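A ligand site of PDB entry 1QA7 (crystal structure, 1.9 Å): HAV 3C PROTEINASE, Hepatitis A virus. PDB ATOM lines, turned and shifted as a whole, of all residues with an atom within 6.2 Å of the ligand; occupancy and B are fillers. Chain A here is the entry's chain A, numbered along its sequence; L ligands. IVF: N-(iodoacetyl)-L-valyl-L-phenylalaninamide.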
ATOM      1  N   GLN A  15      30.948  -2.853  14.472  1.00  0.00           N
ATOM      2  CA  GLN A  15      31.519  -1.858  15.374  1.00  0.00           C
ATOM      3  C   GLN A  15      31.910  -0.709  14.465  1.00  0.00           C
ATOM      4  O   GLN A  15      32.303  -0.936  13.347  1.00  0.00           O
ATOM      5  CB  GLN A  15      32.812  -2.401  16.003  1.00  0.00           C
ATOM      6  CG  GLN A  15      32.634  -3.335  17.230  1.00  0.00           C
ATOM      7  CD  GLN A  15      33.941  -3.620  17.910  1.00  0.00           C
ATOM      8  OE1 GLN A  15      34.895  -4.169  17.316  1.00  0.00           O
ATOM      9  NE2 GLN A  15      34.124  -3.207  19.154  1.00  0.00           N
ATOM     10  N   PHE A  16      31.819   0.531  14.928  1.00  0.00           N
ATOM     11  CA  PHE A  16      32.174   1.624  14.061  1.00  0.00           C
ATOM     12  C   PHE A  16      33.300   2.345  14.747  1.00  0.00           C
ATOM     13  O   PHE A  16      33.240   2.629  15.923  1.00  0.00           O
ATOM     14  CB  PHE A  16      30.970   2.571  13.817  1.00  0.00           C
ATOM     15  CG  PHE A  16      31.326   3.846  13.077  1.00  0.00           C
ATOM     16  CD1 PHE A  16      31.787   4.946  13.749  1.00  0.00           C
ATOM     17  CD2 PHE A  16      31.038   3.990  11.722  1.00  0.00           C
ATOM     18  CE1 PHE A  16      32.177   6.070  13.042  1.00  0.00           C
ATOM     19  CE2 PHE A  16      31.354   5.155  11.041  1.00  0.00           C
ATOM     20  CZ  PHE A  16      31.966   6.161  11.682  1.00  0.00           C
ATOM     21  N   TRP A  27      37.578   2.634  18.215  1.00  0.00           N
ATOM     22  CA  TRP A  27      36.217   2.177  18.057  1.00  0.00           C
ATOM     23  C   TRP A  27      35.349   3.081  18.928  1.00  0.00           C
ATOM     24  O   TRP A  27      35.685   3.394  20.080  1.00  0.00           O
ATOM     25  CB  TRP A  27      36.075   0.685  18.374  1.00  0.00           C
ATOM     26  CG  TRP A  27      36.935  -0.206  17.511  1.00  0.00           C
ATOM     27  CD1 TRP A  27      38.095  -0.825  17.870  1.00  0.00           C
ATOM     28  CD2 TRP A  27      36.683  -0.594  16.171  1.00  0.00           C
ATOM     29  NE1 TRP A  27      38.628  -1.492  16.800  1.00  0.00           N
ATOM     30  CE2 TRP A  27      37.774  -1.378  15.750  1.00  0.00           C
ATOM     31  CE3 TRP A  27      35.701  -0.240  15.242  1.00  0.00           C
ATOM     32  CZ2 TRP A  27      37.892  -1.854  14.444  1.00  0.00           C
ATOM     33  CZ3 TRP A  27      35.795  -0.746  13.969  1.00  0.00           C
ATOM     34  CH2 TRP A  27      36.913  -1.510  13.561  1.00  0.00           C
ATOM     35  N   VAL A  28      34.329   3.660  18.306  1.00  0.00           N
ATOM     36  CA  VAL A  28      33.532   4.664  18.982  1.00  0.00           C
ATOM     37  C   VAL A  28      32.219   4.045  19.411  1.00  0.00           C
ATOM     38  O   VAL A  28      31.814   4.203  20.546  1.00  0.00           O
ATOM     39  CB  VAL A  28      33.332   5.858  18.017  1.00  0.00           C
ATOM     40  CG1 VAL A  28      32.219   6.753  18.456  1.00  0.00           C
ATOM     41  CG2 VAL A  28      34.614   6.635  17.902  1.00  0.00           C
ATOM     42  N   MET A  29      31.614   3.247  18.534  1.00  0.00           N
ATOM     43  CA  MET A  29      30.350   2.589  18.827  1.00  0.00           C
ATOM     44  C   MET A  29      29.999   1.532  17.777  1.00  0.00           C
ATOM     45  O   MET A  29      30.873   0.954  17.133  1.00  0.00           O
ATOM     46  CB  MET A  29      29.222   3.624  18.880  1.00  0.00           C
ATOM     47  CG  MET A  29      29.160   4.600  17.693  1.00  0.00           C
ATOM     48  SD  MET A  29      27.617   5.589  17.711  1.00  0.00           S
ATOM     49  CE  MET A  29      28.109   7.000  18.650  1.00  0.00           C
ATOM     50  N   ASN A  30      28.693   1.273  17.660  1.00  0.00           N
ATOM     51  CA  ASN A  30      28.131   0.347  16.650  1.00  0.00           C
ATOM     52  C   ASN A  30      27.430   1.026  15.457  1.00  0.00           C
ATOM     53  O   ASN A  30      26.993   2.165  15.546  1.00  0.00           O
ATOM     54  CB  ASN A  30      27.142  -0.625  17.302  1.00  0.00           C
ATOM     55  CG  ASN A  30      27.775  -1.417  18.437  1.00  0.00           C
ATOM     56  OD1 ASN A  30      28.429  -2.440  18.213  1.00  0.00           O
ATOM     57  ND2 ASN A  30      27.643  -0.904  19.642  1.00  0.00           N
ATOM     58  N   HIS A  44      26.555  11.126  15.667  1.00  0.00           N
ATOM     59  CA  HIS A  44      27.424  11.486  16.777  1.00  0.00           C
ATOM     60  C   HIS A  44      28.716  10.705  16.771  1.00  0.00           C
ATOM     61  O   HIS A  44      29.706  11.103  17.372  1.00  0.00           O
ATOM     62  CB  HIS A  44      26.680  11.258  18.048  1.00  0.00           C
ATOM     63  CG  HIS A  44      25.216  11.556  17.934  1.00  0.00           C
ATOM     64  ND1 HIS A  44      24.396  10.897  17.026  1.00  0.00           N
ATOM     65  CD2 HIS A  44      24.468  12.553  18.464  1.00  0.00           C
ATOM     66  CE1 HIS A  44      23.201  11.448  17.047  1.00  0.00           C
ATOM     67  NE2 HIS A  44      23.195  12.436  17.925  1.00  0.00           N
ATOM     68  N   THR A 122      26.381  -4.114  21.352  1.00  0.00           N
ATOM     69  CA  THR A 122      27.690  -4.684  21.535  1.00  0.00           C
ATOM     70  C   THR A 122      28.450  -3.771  22.461  1.00  0.00           C
ATOM     71  O   THR A 122      28.363  -2.546  22.331  1.00  0.00           O
ATOM     72  CB  THR A 122      28.442  -4.622  20.201  1.00  0.00           C
ATOM     73  OG1 THR A 122      28.246  -5.838  19.469  1.00  0.00           O
ATOM     74  CG2 THR A 122      29.900  -4.317  20.380  1.00  0.00           C
ATOM     75  N   VAL A 123      29.234  -4.339  23.354  1.00  0.00           N
ATOM     76  CA  VAL A 123      30.187  -3.538  24.089  1.00  0.00           C
ATOM     77  C   VAL A 123      31.507  -4.200  23.982  1.00  0.00           C
ATOM     78  O   VAL A 123      31.646  -5.393  24.304  1.00  0.00           O
ATOM     79  CB  VAL A 123      29.849  -3.186  25.497  1.00  0.00           C
ATOM     80  CG1 VAL A 123      31.120  -2.894  26.221  1.00  0.00           C
ATOM     81  CG2 VAL A 123      29.019  -1.862  25.476  1.00  0.00           C
ATOM     82  N   ASN A 124      32.405  -3.452  23.363  1.00  0.00           N
ATOM     83  CA  ASN A 124      33.674  -3.934  22.841  1.00  0.00           C
ATOM     84  C   ASN A 124      33.912  -5.394  22.680  1.00  0.00           C
ATOM     85  O   ASN A 124      34.433  -6.070  23.562  1.00  0.00           O
ATOM     86  CB  ASN A 124      34.872  -3.019  22.960  1.00  0.00           C
ATOM     87  CG  ASN A 124      35.796  -3.092  21.748  1.00  0.00           C
ATOM     88  OD1 ASN A 124      35.951  -4.157  21.142  1.00  0.00           O
ATOM     89  ND2 ASN A 124      36.466  -1.981  21.448  1.00  0.00           N
ATOM     90  N   GLY A 125      33.372  -5.904  21.573  1.00  0.00           N
ATOM     91  CA  GLY A 125      33.393  -7.301  21.268  1.00  0.00           C
ATOM     92  C   GLY A 125      32.020  -7.742  21.667  1.00  0.00           C
ATOM     93  O   GLY A 125      31.127  -7.789  20.832  1.00  0.00           O
ATOM     94  N   HIS A 145      24.079  12.194  28.304  1.00  0.00           N
ATOM     95  CA  HIS A 145      24.939  11.087  27.836  1.00  0.00           C
ATOM     96  C   HIS A 145      26.297  10.974  28.604  1.00  0.00           C
ATOM     97  O   HIS A 145      26.396  11.413  29.744  1.00  0.00           O
ATOM     98  CB  HIS A 145      25.081  11.101  26.274  1.00  0.00           C
ATOM     99  CG  HIS A 145      25.730   9.883  25.699  1.00  0.00           C
ATOM    100  ND1 HIS A 145      25.444   8.601  26.141  1.00  0.00           N
ATOM    101  CD2 HIS A 145      26.649   9.743  24.710  1.00  0.00           C
ATOM    102  CE1 HIS A 145      26.184   7.731  25.467  1.00  0.00           C
ATOM    103  NE2 HIS A 145      26.926   8.404  24.599  1.00  0.00           N
ATOM    104  N   LYS A 146      27.344  10.407  27.986  1.00  0.00           N
ATOM    105  CA  LYS A 146      28.641  10.162  28.680  1.00  0.00           C
ATOM    106  C   LYS A 146      29.980  10.774  28.127  1.00  0.00           C
ATOM    107  O   LYS A 146      30.372  10.531  26.982  1.00  0.00           O
ATOM    108  CB  LYS A 146      28.802   8.673  28.963  1.00  0.00           C
ATOM    109  CG  LYS A 146      29.945   8.337  29.918  1.00  0.00           C
ATOM    110  CD  LYS A 146      31.269   8.202  29.168  1.00  0.00           C
ATOM    111  CE  LYS A 146      32.422   8.395  30.130  1.00  0.00           C
ATOM    112  NZ  LYS A 146      31.863   8.460  31.502  1.00  0.00           N
ATOM    113  N   LYS A 147      30.684  11.504  29.015  1.00  0.00           N
ATOM    114  CA  LYS A 147      31.991  12.194  28.812  1.00  0.00           C
ATOM    115  C   LYS A 147      32.271  12.914  30.168  1.00  0.00           C
ATOM    116  O   LYS A 147      31.509  13.799  30.551  1.00  0.00           O
ATOM    117  CB  LYS A 147      31.893  13.312  27.755  1.00  0.00           C
ATOM    118  CG  LYS A 147      31.674  12.898  26.317  1.00  0.00           C
ATOM    119  CD  LYS A 147      32.930  12.302  25.689  1.00  0.00           C
ATOM    120  CE  LYS A 147      32.596  11.379  24.506  1.00  0.00           C
ATOM    121  NZ  LYS A 147      33.792  10.727  23.918  1.00  0.00           N
ATOM    122  N   LEU A 168      25.851   1.024  28.922  1.00  0.00           N
ATOM    123  CA  LEU A 168      27.241   1.417  28.984  1.00  0.00           C
ATOM    124  C   LEU A 168      27.579   2.169  27.736  1.00  0.00           C
ATOM    125  O   LEU A 168      26.889   2.027  26.731  1.00  0.00           O
ATOM    126  CB  LEU A 168      28.106   0.176  29.034  1.00  0.00           C
ATOM    127  CG  LEU A 168      27.393  -0.842  29.924  1.00  0.00           C
ATOM    128  CD1 LEU A 168      27.793  -2.273  29.583  1.00  0.00           C
ATOM    129  CD2 LEU A 168      27.578  -0.542  31.409  1.00  0.00           C
ATOM    130  N   PRO A 169      28.628   2.966  27.793  1.00  0.00           N
ATOM    131  CA  PRO A 169      29.057   3.691  26.620  1.00  0.00           C
ATOM    132  C   PRO A 169      29.506   2.609  25.657  1.00  0.00           C
ATOM    133  O   PRO A 169      29.722   1.469  26.053  1.00  0.00           O
ATOM    134  CB  PRO A 169      30.260   4.508  27.097  1.00  0.00           C
ATOM    135  CG  PRO A 169      30.136   4.579  28.550  1.00  0.00           C
ATOM    136  CD  PRO A 169      29.326   3.392  29.015  1.00  0.00           C
ATOM    137  N   GLY A 170      29.461   2.928  24.363  1.00  0.00           N
ATOM    138  CA  GLY A 170      29.743   1.957  23.320  1.00  0.00           C
ATOM    139  C   GLY A 170      28.453   1.329  22.789  1.00  0.00           C
ATOM    140  O   GLY A 170      28.455   0.696  21.727  1.00  0.00           O
ATOM    141  N   MET A 171      27.364   1.455  23.543  1.00  0.00           N
ATOM    142  CA  MET A 171      26.099   0.856  23.111  1.00  0.00           C
ATOM    143  C   MET A 171      25.411   1.589  21.939  1.00  0.00           C
ATOM    144  O   MET A 171      24.516   1.067  21.300  1.00  0.00           O
ATOM    145  CB  MET A 171      25.140   0.755  24.283  1.00  0.00           C
ATOM    146  CG  MET A 171      25.620  -0.177  25.321  1.00  0.00           C
ATOM    147  SD  MET A 171      24.295  -0.597  26.393  1.00  0.00           S
ATOM    148  CE  MET A 171      23.633   1.067  26.732  1.00  0.00           C
ATOM    149  N   CYS A 172      25.775   2.831  21.692  1.00  0.00           N
ATOM    150  CA  CYS A 172      25.109   3.585  20.653  1.00  0.00           C
ATOM    151  C   CYS A 172      25.271   2.903  19.338  1.00  0.00           C
ATOM    152  O   CYS A 172      26.306   2.299  19.068  1.00  0.00           O
ATOM    153  CB  CYS A 172      25.734   4.956  20.571  1.00  0.00           C
ATOM    154  SG  CYS A 172      25.451   5.922  22.077  1.00  0.00           S
ATOM    155  N   GLY A 173      24.234   2.962  18.507  1.00  0.00           N
ATOM    156  CA  GLY A 173      24.242   2.321  17.199  1.00  0.00           C
ATOM    157  C   GLY A 173      23.604   0.943  17.213  1.00  0.00           C
ATOM    158  O   GLY A 173      23.363   0.377  16.171  1.00  0.00           O
ATOM    159  N   HIS A 191      19.909   3.177  19.102  1.00  0.00           N
ATOM    160  CA  HIS A 191      20.274   3.804  20.349  1.00  0.00           C
ATOM    161  C   HIS A 191      21.289   4.929  20.201  1.00  0.00           C
ATOM    162  O   HIS A 191      22.312   4.765  19.503  1.00  0.00           O
ATOM    163  CB  HIS A 191      20.755   2.786  21.319  1.00  0.00           C
ATOM    164  CG  HIS A 191      21.169   3.366  22.620  1.00  0.00           C
ATOM    165  ND1 HIS A 191      20.305   3.485  23.681  1.00  0.00           N
ATOM    166  CD2 HIS A 191      22.360   3.853  23.048  1.00  0.00           C
ATOM    167  CE1 HIS A 191      20.943   4.002  24.716  1.00  0.00           C
ATOM    168  NE2 HIS A 191      22.202   4.221  24.371  1.00  0.00           N
ATOM    169  N   VAL A 192      20.964   6.080  20.799  1.00  0.00           N
ATOM    170  CA  VAL A 192      21.760   7.291  20.636  1.00  0.00           C
ATOM    171  C   VAL A 192      22.219   7.931  21.914  1.00  0.00           C
ATOM    172  O   VAL A 192      23.053   8.809  21.880  1.00  0.00           O
ATOM    173  CB  VAL A 192      21.023   8.365  19.767  1.00  0.00           C
ATOM    174  CG1 VAL A 192      21.009   7.981  18.315  1.00  0.00           C
ATOM    175  CG2 VAL A 192      19.585   8.598  20.254  1.00  0.00           C
ATOM    176  N   ALA A 193      21.688   7.534  23.054  1.00  0.00           N
ATOM    177  CA  ALA A 193      22.063   8.227  24.300  1.00  0.00           C
ATOM    178  C   ALA A 193      21.595   7.456  25.537  1.00  0.00           C
ATOM    179  O   ALA A 193      20.577   6.764  25.507  1.00  0.00           O
ATOM    180  CB  ALA A 193      21.474   9.631  24.305  1.00  0.00           C
ATOM    181  N   GLY A 194      22.379   7.530  26.606  1.00  0.00           N
ATOM    182  CA  GLY A 194      22.106   6.752  27.795  1.00  0.00           C
ATOM    183  C   GLY A 194      22.701   7.378  29.042  1.00  0.00           C
ATOM    184  O   GLY A 194      23.920   7.358  29.244  1.00  0.00           O
HETATM  185  C1  IVF L   1      28.134   5.024  22.984  1.00  0.00           C
HETATM  186  O1  IVF L   1      28.255   4.068  22.245  1.00  0.00           O
HETATM  187  CH3 IVF L   1      26.750   5.437  23.460  1.00  0.00           C
HETATM  188  N2  IVF L   1      29.184   5.763  23.385  1.00  0.00           N
HETATM  189  CA2 IVF L   1      30.556   5.620  22.871  1.00  0.00           C
HETATM  190  C2  IVF L   1      31.489   4.756  23.727  1.00  0.00           C
HETATM  191  O2  IVF L   1      31.797   5.170  24.841  1.00  0.00           O
HETATM  192  CB2 IVF L   1      31.240   7.014  22.735  1.00  0.00           C
HETATM  193  CG1 IVF L   1      32.547   6.878  21.953  1.00  0.00           C
HETATM  194  CG2 IVF L   1      30.280   8.064  22.105  1.00  0.00           C
HETATM  195  N   IVF L   1      32.014   3.636  23.169  1.00  0.00           N
HETATM  196  CA  IVF L   1      32.865   2.650  23.874  1.00  0.00           C
HETATM  197  C   IVF L   1      33.785   3.252  24.928  1.00  0.00           C
HETATM  198  O   IVF L   1      34.502   4.207  24.595  1.00  0.00           O
HETATM  199  CB  IVF L   1      33.732   1.810  22.916  1.00  0.00           C
HETATM  200  CG  IVF L   1      32.947   0.910  21.991  1.00  0.00           C
HETATM  201  CD1 IVF L   1      31.924   0.094  22.462  1.00  0.00           C
HETATM  202  CD2 IVF L   1      33.296   0.806  20.642  1.00  0.00           C
HETATM  203  CE1 IVF L   1      31.211  -0.713  21.596  1.00  0.00           C
HETATM  204  CE2 IVF L   1      32.607  -0.032  19.789  1.00  0.00           C
HETATM  205  CZ  IVF L   1      31.569  -0.800  20.270  1.00  0.00           C
HETATM  206  NXT IVF L   1      33.723   2.753  26.282  1.00  0.00           N
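An oxygen (O1) of the ligand sits at hydrogen-bond distance from the backbone NH (N) of Cys 172 (2.8 Å). The side-chain sulfur of Cys 172 is bonded to a carbon (CH3) of the ligand, at 2.0 Å. A nitrogen (N) of the ligand is in hydrogen-bond range of the backbone carbonyl oxygen (O) of Val 28, 2.7 Å away. The backbone NH of Gly 170 lies within hydrogen-bond range of an oxygen (O1) of the ligand, at 2.7 Å. The backbone NH (N) of Met 171 is in hydrogen-bond range of an oxygen (O1) of the ligand.
Gln 15 touches the ligand (NE2 to CE2, 3.6 Å). Trp 27 touches the ligand. Met 29 touches the ligand. Asn 30 touches the ligand. Thr 122 touches the ligand. CA of Val 123 touches CE1 of the ligand (3.9 Å). Asn 124 touches the ligand (N to CE1, 3.5 Å). CE1 of His 145 touches CH3 of the ligand (3.1 Å). Pro 169 touches the ligand (CB to O2, 2.8 Å). Hydrophobic or aromatic side chains within 4 Å of the ligand: Trp 27, Val 28, Met 29, His 145 and Pro 169.
O of Cys 172 is in hydrogen-bond range of N of Asn 30, at 3.0 Å. The backbone NH (N) of Val 28 is in hydrogen-bond range of the backbone carbonyl oxygen (O) of Phe 16 (2.8 Å). The side-chain amide nitrogen (ND2) of Asn 30 sits at hydrogen-bond distance from the backbone carbonyl oxygen (O) of Gly 170 (2.8 Å). SD of Met 171 sits close to N of Leu 168 (3.4 Å). ND1 of His 145 lies within hydrogen-bond range of N of Gly 194. N of Phe 16 is in hydrogen-bond range of O of Met 29 (2.4 Å). ND2 of Asn 30 lies within hydrogen-bond range of O of Thr 122 (3.2 Å). The side-chain amide nitrogen of Gln 15 is in hydrogen-bond range of the side-chain amide oxygen of Asn 124 (2.9 Å).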
